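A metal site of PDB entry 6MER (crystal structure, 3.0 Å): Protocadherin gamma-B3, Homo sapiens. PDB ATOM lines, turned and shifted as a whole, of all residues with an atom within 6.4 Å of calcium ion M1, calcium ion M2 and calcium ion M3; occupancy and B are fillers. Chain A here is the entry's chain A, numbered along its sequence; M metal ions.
Of the 26 residues printed, 6 come within 4 Å of calcium ion M1.
Of the 26 residues printed, 6 come within 4 Å of calcium ion M2.
The side-chain carboxylate (OD1) of Asp 61 is bound to calcium ion M3 (2.5 Å).
Calcium ion M3 is bound by OD2 of Asp 98, 2.5 Å away.
Calcium ion M3 is bound by the side-chain carboxylate (OE1) of Glu 63 (2.6 Å).
Calcium ion M3 is bound by the side-chain carboxylate (OE2) of Glu 10 (2.6 Å).
Slightly farther from calcium ion M3 lies OE1 of Glu 9 (3.0 Å).
The backbone carbonyl oxygen of Gln 94 sits at hydrogen-bond distance from the backbone NH of Glu 9, at 3.2 Å.
OE1 of Glu 63 lies close to OD1 of Asn 99 (3.2 Å).
The side-chain carboxylate of Glu 63 lies close to the guanidinium group of Arg 62 (3.3 Å).
The side-chain carboxylate (OD2) of Asp 61 is in hydrogen-bond range of the backbone NH (N) of Glu 64.
The side-chain amide oxygen (OD1) of Asn 99 lies close to the side-chain carboxylate (OD1) of Asp 98 (3.1 Å).
The guanidinium group (NE) of Arg 62 sits close to the side-chain carboxylate (OD1) of Asp 95 (2.9 Å).
N of Glu 10 lies within hydrogen-bond range of O of Ile 60, 2.9 Å away.
The backbone NH (N) of Asp 186 lies within hydrogen-bond range of the side-chain amide oxygen (OE1) of Gln 138, 3.1 Å away.
Of the 26 residues printed, 6 come within 4 Å of calcium ion M3.
Calcium ion M1 is bound by OD1 of Asn 97 (2.5 Å), O of Asn 135 (2.5 Å), OD1 of Asp 129 (2.6 Å), O of Asn 99 (2.6 Å), OD1 of Asp 131 (2.6 Å), OD2 of Asp 129 (2.6 Å) and OD2 of Asp 186 (2.6 Å).
The side-chain carboxylate (OE2) of Glu 9 binds calcium ion M2, at 2.4 Å.
Calcium ion M2 is bound by OD2 of Asp 131, at 2.4 Å.
The side-chain carboxylate (OE2) of Glu 63 binds calcium ion M2.
OD1 of Asp 95 is bound to calcium ion M2, 2.5 Å away.
The backbone carbonyl oxygen (O) of Ile 96 binds calcium ion M2, 2.6 Å away.
OD1 of Asp 98 is bound to calcium ion M2.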
ATOM      1  N   GLU A   9       6.275 -20.411   7.865  1.00  0.00           N
ATOM      2  CA  GLU A   9       5.820 -21.379   8.847  1.00  0.00           C
ATOM      3  C   GLU A   9       6.715 -21.371  10.082  1.00  0.00           C
ATOM      4  O   GLU A   9       7.751 -20.711  10.124  1.00  0.00           O
ATOM      5  CB  GLU A   9       5.783 -22.782   8.238  1.00  0.00           C
ATOM      6  CG  GLU A   9       7.114 -23.238   7.680  1.00  0.00           C
ATOM      7  CD  GLU A   9       7.206 -24.747   7.548  1.00  0.00           C
ATOM      8  OE1 GLU A   9       6.413 -25.451   8.206  1.00  0.00           O
ATOM      9  OE2 GLU A   9       8.063 -25.221   6.778  1.00  0.00           O
ATOM     10  N   GLU A  10       6.290 -22.117  11.097  1.00  0.00           N
ATOM     11  CA  GLU A  10       7.049 -22.309  12.328  1.00  0.00           C
ATOM     12  C   GLU A  10       7.332 -20.973  13.027  1.00  0.00           C
ATOM     13  O   GLU A  10       8.453 -20.697  13.456  1.00  0.00           O
ATOM     14  CB  GLU A  10       8.344 -23.078  12.059  1.00  0.00           C
ATOM     15  CG  GLU A  10       8.160 -24.404  11.340  1.00  0.00           C
ATOM     16  CD  GLU A  10       7.537 -25.472  12.209  1.00  0.00           C
ATOM     17  OE1 GLU A  10       7.360 -25.242  13.423  1.00  0.00           O
ATOM     18  OE2 GLU A  10       7.224 -26.564  11.684  1.00  0.00           O
ATOM     19  N   ARG A  59       1.466 -24.094  16.700  1.00  0.00           N
ATOM     20  CA  ARG A  59       2.575 -24.349  15.791  1.00  0.00           C
ATOM     21  C   ARG A  59       2.071 -24.549  14.367  1.00  0.00           C
ATOM     22  O   ARG A  59       1.163 -25.361  14.128  1.00  0.00           O
ATOM     23  CB  ARG A  59       3.360 -25.579  16.254  1.00  0.00           C
ATOM     24  CG  ARG A  59       4.514 -25.969  15.343  1.00  0.00           C
ATOM     25  CD  ARG A  59       5.337 -27.092  15.948  1.00  0.00           C
ATOM     26  NE  ARG A  59       6.412 -27.527  15.069  1.00  0.00           N
ATOM     27  CZ  ARG A  59       6.346 -28.587  14.271  1.00  0.00           C
ATOM     28  NH1 ARG A  59       5.243 -29.332  14.233  1.00  0.00           N
ATOM     29  NH2 ARG A  59       7.382 -28.911  13.505  1.00  0.00           N
ATOM     30  N   ILE A  60       2.649 -23.816  13.432  1.00  0.00           N
ATOM     31  CA  ILE A  60       2.252 -23.868  12.024  1.00  0.00           C
ATOM     32  C   ILE A  60       3.299 -24.704  11.305  1.00  0.00           C
ATOM     33  O   ILE A  60       4.318 -24.190  10.823  1.00  0.00           O
ATOM     34  CB  ILE A  60       2.102 -22.475  11.417  1.00  0.00           C
ATOM     35  CG1 ILE A  60       1.199 -21.602  12.296  1.00  0.00           C
ATOM     36  CG2 ILE A  60       1.528 -22.568  10.013  1.00  0.00           C
ATOM     37  CD1 ILE A  60      -0.206 -22.133  12.461  1.00  0.00           C
ATOM     38  N   ASP A  61       3.059 -26.006  11.223  1.00  0.00           N
ATOM     39  CA  ASP A  61       3.937 -26.929  10.516  1.00  0.00           C
ATOM     40  C   ASP A  61       3.345 -27.163   9.126  1.00  0.00           C
ATOM     41  O   ASP A  61       2.264 -27.742   8.996  1.00  0.00           O
ATOM     42  CB  ASP A  61       4.089 -28.242  11.279  1.00  0.00           C
ATOM     43  CG  ASP A  61       5.011 -29.227  10.590  1.00  0.00           C
ATOM     44  OD1 ASP A  61       6.247 -29.016  10.630  1.00  0.00           O
ATOM     45  OD2 ASP A  61       4.516 -30.209  10.007  1.00  0.00           O
ATOM     46  N   ARG A  62       4.064 -26.721   8.100  1.00  0.00           N
ATOM     47  CA  ARG A  62       3.545 -26.841   6.735  1.00  0.00           C
ATOM     48  C   ARG A  62       3.493 -28.291   6.278  1.00  0.00           C
ATOM     49  O   ARG A  62       2.676 -28.646   5.416  1.00  0.00           O
ATOM     50  CB  ARG A  62       4.400 -26.014   5.771  1.00  0.00           C
ATOM     51  CG  ARG A  62       3.732 -25.772   4.422  1.00  0.00           C
ATOM     52  CD  ARG A  62       4.774 -25.608   3.325  1.00  0.00           C
ATOM     53  NE  ARG A  62       5.551 -26.823   3.146  1.00  0.00           N
ATOM     54  CZ  ARG A  62       5.177 -27.852   2.393  1.00  0.00           C
ATOM     55  NH1 ARG A  62       4.023 -27.808   1.740  1.00  0.00           N
ATOM     56  NH2 ARG A  62       5.948 -28.923   2.290  1.00  0.00           N
ATOM     57  N   GLU A  63       4.352 -29.155   6.837  1.00  0.00           N
ATOM     58  CA  GLU A  63       4.363 -30.561   6.442  1.00  0.00           C
ATOM     59  C   GLU A  63       3.199 -31.338   7.045  1.00  0.00           C
ATOM     60  O   GLU A  63       2.764 -32.343   6.464  1.00  0.00           O
ATOM     61  CB  GLU A  63       5.689 -31.211   6.841  1.00  0.00           C
ATOM     62  CG  GLU A  63       6.868 -30.824   5.957  1.00  0.00           C
ATOM     63  CD  GLU A  63       7.304 -29.384   6.159  1.00  0.00           C
ATOM     64  OE1 GLU A  63       7.308 -28.912   7.313  1.00  0.00           O
ATOM     65  OE2 GLU A  63       7.658 -28.721   5.161  1.00  0.00           O
ATOM     66  N   GLU A  64       2.685 -30.892   8.185  1.00  0.00           N
ATOM     67  CA  GLU A  64       1.527 -31.555   8.789  1.00  0.00           C
ATOM     68  C   GLU A  64       0.227 -31.129   8.128  1.00  0.00           C
ATOM     69  O   GLU A  64      -0.749 -31.890   8.122  1.00  0.00           O
ATOM     70  CB  GLU A  64       1.486 -31.252  10.292  1.00  0.00           C
ATOM     71  CG  GLU A  64       0.360 -31.944  11.049  1.00  0.00           C
ATOM     72  CD  GLU A  64       0.565 -33.442  11.168  1.00  0.00           C
ATOM     73  OE1 GLU A  64       1.709 -33.903  10.999  1.00  0.00           O
ATOM     74  OE2 GLU A  64      -0.429 -34.163  11.431  1.00  0.00           O
ATOM     75  N   GLN A  94       4.309 -20.068   3.849  1.00  0.00           N
ATOM     76  CA  GLN A  94       5.527 -20.212   3.069  1.00  0.00           C
ATOM     77  C   GLN A  94       6.405 -21.307   3.660  1.00  0.00           C
ATOM     78  O   GLN A  94       6.482 -21.466   4.884  1.00  0.00           O
ATOM     79  CB  GLN A  94       6.287 -18.892   3.017  1.00  0.00           C
ATOM     80  CG  GLN A  94       5.524 -17.775   2.313  1.00  0.00           C
ATOM     81  CD  GLN A  94       6.256 -16.442   2.370  1.00  0.00           C
ATOM     82  OE1 GLN A  94       7.090 -16.215   3.249  1.00  0.00           O
ATOM     83  NE2 GLN A  94       5.946 -15.564   1.430  1.00  0.00           N
ATOM     84  N   ASP A  95       7.059 -22.062   2.789  1.00  0.00           N
ATOM     85  CA  ASP A  95       7.879 -23.194   3.197  1.00  0.00           C
ATOM     86  C   ASP A  95       9.284 -22.733   3.550  1.00  0.00           C
ATOM     87  O   ASP A  95       9.919 -22.000   2.779  1.00  0.00           O
ATOM     88  CB  ASP A  95       7.935 -24.243   2.093  1.00  0.00           C
ATOM     89  CG  ASP A  95       8.825 -25.419   2.434  1.00  0.00           C
ATOM     90  OD1 ASP A  95       8.433 -26.241   3.290  1.00  0.00           O
ATOM     91  OD2 ASP A  95       9.931 -25.525   1.852  1.00  0.00           O
ATOM     92  N   ILE A  96       9.769 -23.163   4.716  1.00  0.00           N
ATOM     93  CA  ILE A  96      11.152 -22.920   5.130  1.00  0.00           C
ATOM     94  C   ILE A  96      11.873 -24.264   5.155  1.00  0.00           C
ATOM     95  O   ILE A  96      11.264 -25.316   5.382  1.00  0.00           O
ATOM     96  CB  ILE A  96      11.234 -22.224   6.507  1.00  0.00           C
ATOM     97  CG1 ILE A  96      10.720 -23.141   7.613  1.00  0.00           C
ATOM     98  CG2 ILE A  96      10.470 -20.912   6.488  1.00  0.00           C
ATOM     99  CD1 ILE A  96      10.827 -22.553   9.000  1.00  0.00           C
ATOM    100  N   ASN A  97      13.180 -24.217   4.910  1.00  0.00           N
ATOM    101  CA  ASN A  97      13.996 -25.428   4.859  1.00  0.00           C
ATOM    102  C   ASN A  97      14.378 -25.826   6.279  1.00  0.00           C
ATOM    103  O   ASN A  97      15.502 -25.600   6.754  1.00  0.00           O
ATOM    104  CB  ASN A  97      15.230 -25.201   3.987  1.00  0.00           C
ATOM    105  CG  ASN A  97      16.019 -26.473   3.768  1.00  0.00           C
ATOM    106  OD1 ASN A  97      15.495 -27.586   3.936  1.00  0.00           O
ATOM    107  ND2 ASN A  97      17.287 -26.340   3.399  1.00  0.00           N
ATOM    108  N   ASP A  98      13.417 -26.433   6.976  1.00  0.00           N
ATOM    109  CA  ASP A  98      13.610 -26.871   8.350  1.00  0.00           C
ATOM    110  C   ASP A  98      13.709 -28.383   8.479  1.00  0.00           C
ATOM    111  O   ASP A  98      13.961 -28.879   9.579  1.00  0.00           O
ATOM    112  CB  ASP A  98      12.475 -26.355   9.234  1.00  0.00           C
ATOM    113  CG  ASP A  98      11.094 -26.699   8.692  1.00  0.00           C
ATOM    114  OD1 ASP A  98      11.012 -27.280   7.586  1.00  0.00           O
ATOM    115  OD2 ASP A  98      10.096 -26.397   9.376  1.00  0.00           O
ATOM    116  N   ASN A  99      13.538 -29.123   7.386  1.00  0.00           N
ATOM    117  CA  ASN A  99      13.629 -30.573   7.405  1.00  0.00           C
ATOM    118  C   ASN A  99      14.787 -31.029   6.528  1.00  0.00           C
ATOM    119  O   ASN A  99      14.894 -30.601   5.369  1.00  0.00           O
ATOM    120  CB  ASN A  99      12.318 -31.219   6.922  1.00  0.00           C
ATOM    121  CG  ASN A  99      11.170 -30.988   7.889  1.00  0.00           C
ATOM    122  OD1 ASN A  99      10.207 -30.290   7.574  1.00  0.00           O
ATOM    123  ND2 ASN A  99      11.266 -31.586   9.069  1.00  0.00           N
ATOM    124  N   PRO A 100      15.669 -31.887   7.033  1.00  0.00           N
ATOM    125  CA  PRO A 100      16.783 -32.373   6.220  1.00  0.00           C
ATOM    126  C   PRO A 100      16.344 -33.544   5.350  1.00  0.00           C
ATOM    127  O   PRO A 100      15.340 -34.203   5.646  1.00  0.00           O
ATOM    128  CB  PRO A 100      17.812 -32.804   7.262  1.00  0.00           C
ATOM    129  CG  PRO A 100      16.972 -33.268   8.414  1.00  0.00           C
ATOM    130  CD  PRO A 100      15.744 -32.390   8.411  1.00  0.00           C
ATOM    131  N   PRO A 101      17.083 -33.819   4.275  1.00  0.00           N
ATOM    132  CA  PRO A 101      16.779 -35.007   3.471  1.00  0.00           C
ATOM    133  C   PRO A 101      17.040 -36.282   4.261  1.00  0.00           C
ATOM    134  O   PRO A 101      17.773 -36.302   5.245  1.00  0.00           O
ATOM    135  CB  PRO A 101      17.736 -34.891   2.281  1.00  0.00           C
ATOM    136  CG  PRO A 101      18.152 -33.458   2.249  1.00  0.00           C
ATOM    137  CD  PRO A 101      18.151 -33.015   3.678  1.00  0.00           C
ATOM    138  N   ASP A 129      12.471 -35.476   0.824  1.00  0.00           N
ATOM    139  CA  ASP A 129      12.516 -34.222   1.572  1.00  0.00           C
ATOM    140  C   ASP A 129      11.077 -33.781   1.836  1.00  0.00           C
ATOM    141  O   ASP A 129      10.315 -33.584   0.869  1.00  0.00           O
ATOM    142  CB  ASP A 129      13.289 -33.145   0.801  1.00  0.00           C
ATOM    143  CG  ASP A 129      14.002 -32.175   1.721  1.00  0.00           C
ATOM    144  OD1 ASP A 129      13.574 -32.022   2.879  1.00  0.00           O
ATOM    145  OD2 ASP A 129      14.996 -31.565   1.277  1.00  0.00           O
ATOM    146  N   PRO A 130      10.667 -33.627   3.091  1.00  0.00           N
ATOM    147  CA  PRO A 130       9.277 -33.242   3.366  1.00  0.00           C
ATOM    148  C   PRO A 130       8.906 -31.852   2.869  1.00  0.00           C
ATOM    149  O   PRO A 130       7.709 -31.559   2.734  1.00  0.00           O
ATOM    150  CB  PRO A 130       9.175 -33.325   4.894  1.00  0.00           C
ATOM    151  CG  PRO A 130      10.318 -34.197   5.313  1.00  0.00           C
ATOM    152  CD  PRO A 130      11.411 -33.916   4.330  1.00  0.00           C
ATOM    153  N   ASP A 131       9.883 -31.002   2.590  1.00  0.00           N
ATOM    154  CA  ASP A 131       9.600 -29.639   2.136  1.00  0.00           C
ATOM    155  C   ASP A 131       9.231 -29.644   0.657  1.00  0.00           C
ATOM    156  O   ASP A 131       9.180 -30.687  -0.001  1.00  0.00           O
ATOM    157  CB  ASP A 131      10.806 -28.736   2.401  1.00  0.00           C
ATOM    158  CG  ASP A 131      11.381 -28.929   3.793  1.00  0.00           C
ATOM    159  OD1 ASP A 131      12.121 -29.911   3.992  1.00  0.00           O
ATOM    160  OD2 ASP A 131      11.095 -28.101   4.672  1.00  0.00           O
ATOM    161  N   VAL A 132       8.960 -28.457   0.119  1.00  0.00           N
ATOM    162  CA  VAL A 132       8.619 -28.274  -1.287  1.00  0.00           C
ATOM    163  C   VAL A 132       9.479 -27.166  -1.864  1.00  0.00           C
ATOM    164  O   VAL A 132      10.206 -26.467  -1.151  1.00  0.00           O
ATOM    165  CB  VAL A 132       7.121 -27.964  -1.487  1.00  0.00           C
ATOM    166  CG1 VAL A 132       6.258 -29.129  -1.047  1.00  0.00           C
ATOM    167  CG2 VAL A 132       6.736 -26.699  -0.729  1.00  0.00           C
ATOM    168  N   VAL A 134      12.409 -25.158  -3.769  1.00  0.00           N
ATOM    169  CA  VAL A 134      13.861 -25.290  -3.762  1.00  0.00           C
ATOM    170  C   VAL A 134      14.355 -25.996  -2.508  1.00  0.00           C
ATOM    171  O   VAL A 134      15.454 -26.555  -2.513  1.00  0.00           O
ATOM    172  CB  VAL A 134      14.534 -23.915  -3.922  1.00  0.00           C
ATOM    173  CG1 VAL A 134      14.116 -23.262  -5.232  1.00  0.00           C
ATOM    174  CG2 VAL A 134      14.191 -23.015  -2.740  1.00  0.00           C
ATOM    175  N   ASN A 135      13.570 -25.994  -1.433  1.00  0.00           N
ATOM    176  CA  ASN A 135      13.947 -26.693  -0.214  1.00  0.00           C
ATOM    177  C   ASN A 135      13.819 -28.202  -0.348  1.00  0.00           C
ATOM    178  O   ASN A 135      14.191 -28.920   0.591  1.00  0.00           O
ATOM    179  CB  ASN A 135      13.103 -26.202   0.953  1.00  0.00           C
ATOM    180  CG  ASN A 135      13.172 -24.704   1.143  1.00  0.00           C
ATOM    181  OD1 ASN A 135      14.214 -24.088   0.920  1.00  0.00           O
ATOM    182  ND2 ASN A 135      12.053 -24.099   1.536  1.00  0.00           N
ATOM    183  N   SER A 136      13.301 -28.699  -1.470  1.00  0.00           N
ATOM    184  CA  SER A 136      13.183 -30.129  -1.719  1.00  0.00           C
ATOM    185  C   SER A 136      14.068 -30.628  -2.854  1.00  0.00           C
ATOM    186  O   SER A 136      14.349 -31.824  -2.910  1.00  0.00           O
ATOM    187  CB  SER A 136      11.731 -30.509  -2.017  1.00  0.00           C
ATOM    188  OG  SER A 136      11.587 -31.900  -2.204  1.00  0.00           O
ATOM    189  N   GLN A 138      17.208 -31.741  -4.589  1.00  0.00           N
ATOM    190  CA  GLN A 138      18.398 -32.324  -3.998  1.00  0.00           C
ATOM    191  C   GLN A 138      19.574 -32.299  -4.960  1.00  0.00           C
ATOM    192  O   GLN A 138      19.406 -32.379  -6.183  1.00  0.00           O
ATOM    193  CB  GLN A 138      18.136 -33.778  -3.559  1.00  0.00           C
ATOM    194  CG  GLN A 138      17.012 -33.918  -2.547  1.00  0.00           C
ATOM    195  CD  GLN A 138      17.319 -33.225  -1.241  1.00  0.00           C
ATOM    196  OE1 GLN A 138      18.485 -33.016  -0.884  1.00  0.00           O
ATOM    197  NE2 GLN A 138      16.271 -32.864  -0.507  1.00  0.00           N
ATOM    198  N   ASP A 186      20.040 -30.478  -0.045  1.00  0.00           N
ATOM    199  CA  ASP A 186      18.968 -29.707  -0.651  1.00  0.00           C
ATOM    200  C   ASP A 186      19.423 -28.280  -0.926  1.00  0.00           C
ATOM    201  O   ASP A 186      20.460 -27.819  -0.447  1.00  0.00           O
ATOM    202  CB  ASP A 186      17.725 -29.726   0.233  1.00  0.00           C
ATOM    203  CG  ASP A 186      18.003 -29.305   1.667  1.00  0.00           C
ATOM    204  OD1 ASP A 186      19.131 -28.833   1.949  1.00  0.00           O
ATOM    205  OD2 ASP A 186      17.100 -29.437   2.514  1.00  0.00           O
ATOM    206  N   ARG A 192      20.632 -28.255   4.351  1.00  0.00           N
ATOM    207  CA  ARG A 192      20.677 -29.449   5.180  1.00  0.00           C
ATOM    208  C   ARG A 192      21.105 -30.655   4.353  1.00  0.00           C
ATOM    209  O   ARG A 192      20.785 -30.760   3.163  1.00  0.00           O
ATOM    210  CB  ARG A 192      19.318 -29.705   5.822  1.00  0.00           C
ATOM    211  CG  ARG A 192      18.816 -28.531   6.650  1.00  0.00           C
ATOM    212  CD  ARG A 192      17.528 -28.867   7.397  1.00  0.00           C
ATOM    213  NE  ARG A 192      17.075 -27.750   8.205  1.00  0.00           N
ATOM    214  CZ  ARG A 192      17.484 -27.512   9.446  1.00  0.00           C
ATOM    215  NH1 ARG A 192      18.361 -28.314  10.025  1.00  0.00           N
ATOM    216  NH2 ARG A 192      17.024 -26.466  10.118  1.00  0.00           N
HETATM  217 CA    CA M   1      14.518 -29.637   2.992  1.00  0.00          CA
HETATM  218 CA    CA M   2       9.239 -26.919   5.591  1.00  0.00          CA
HETATM  219 CA    CA M   3       7.951 -27.653   9.462  1.00  0.00          CA
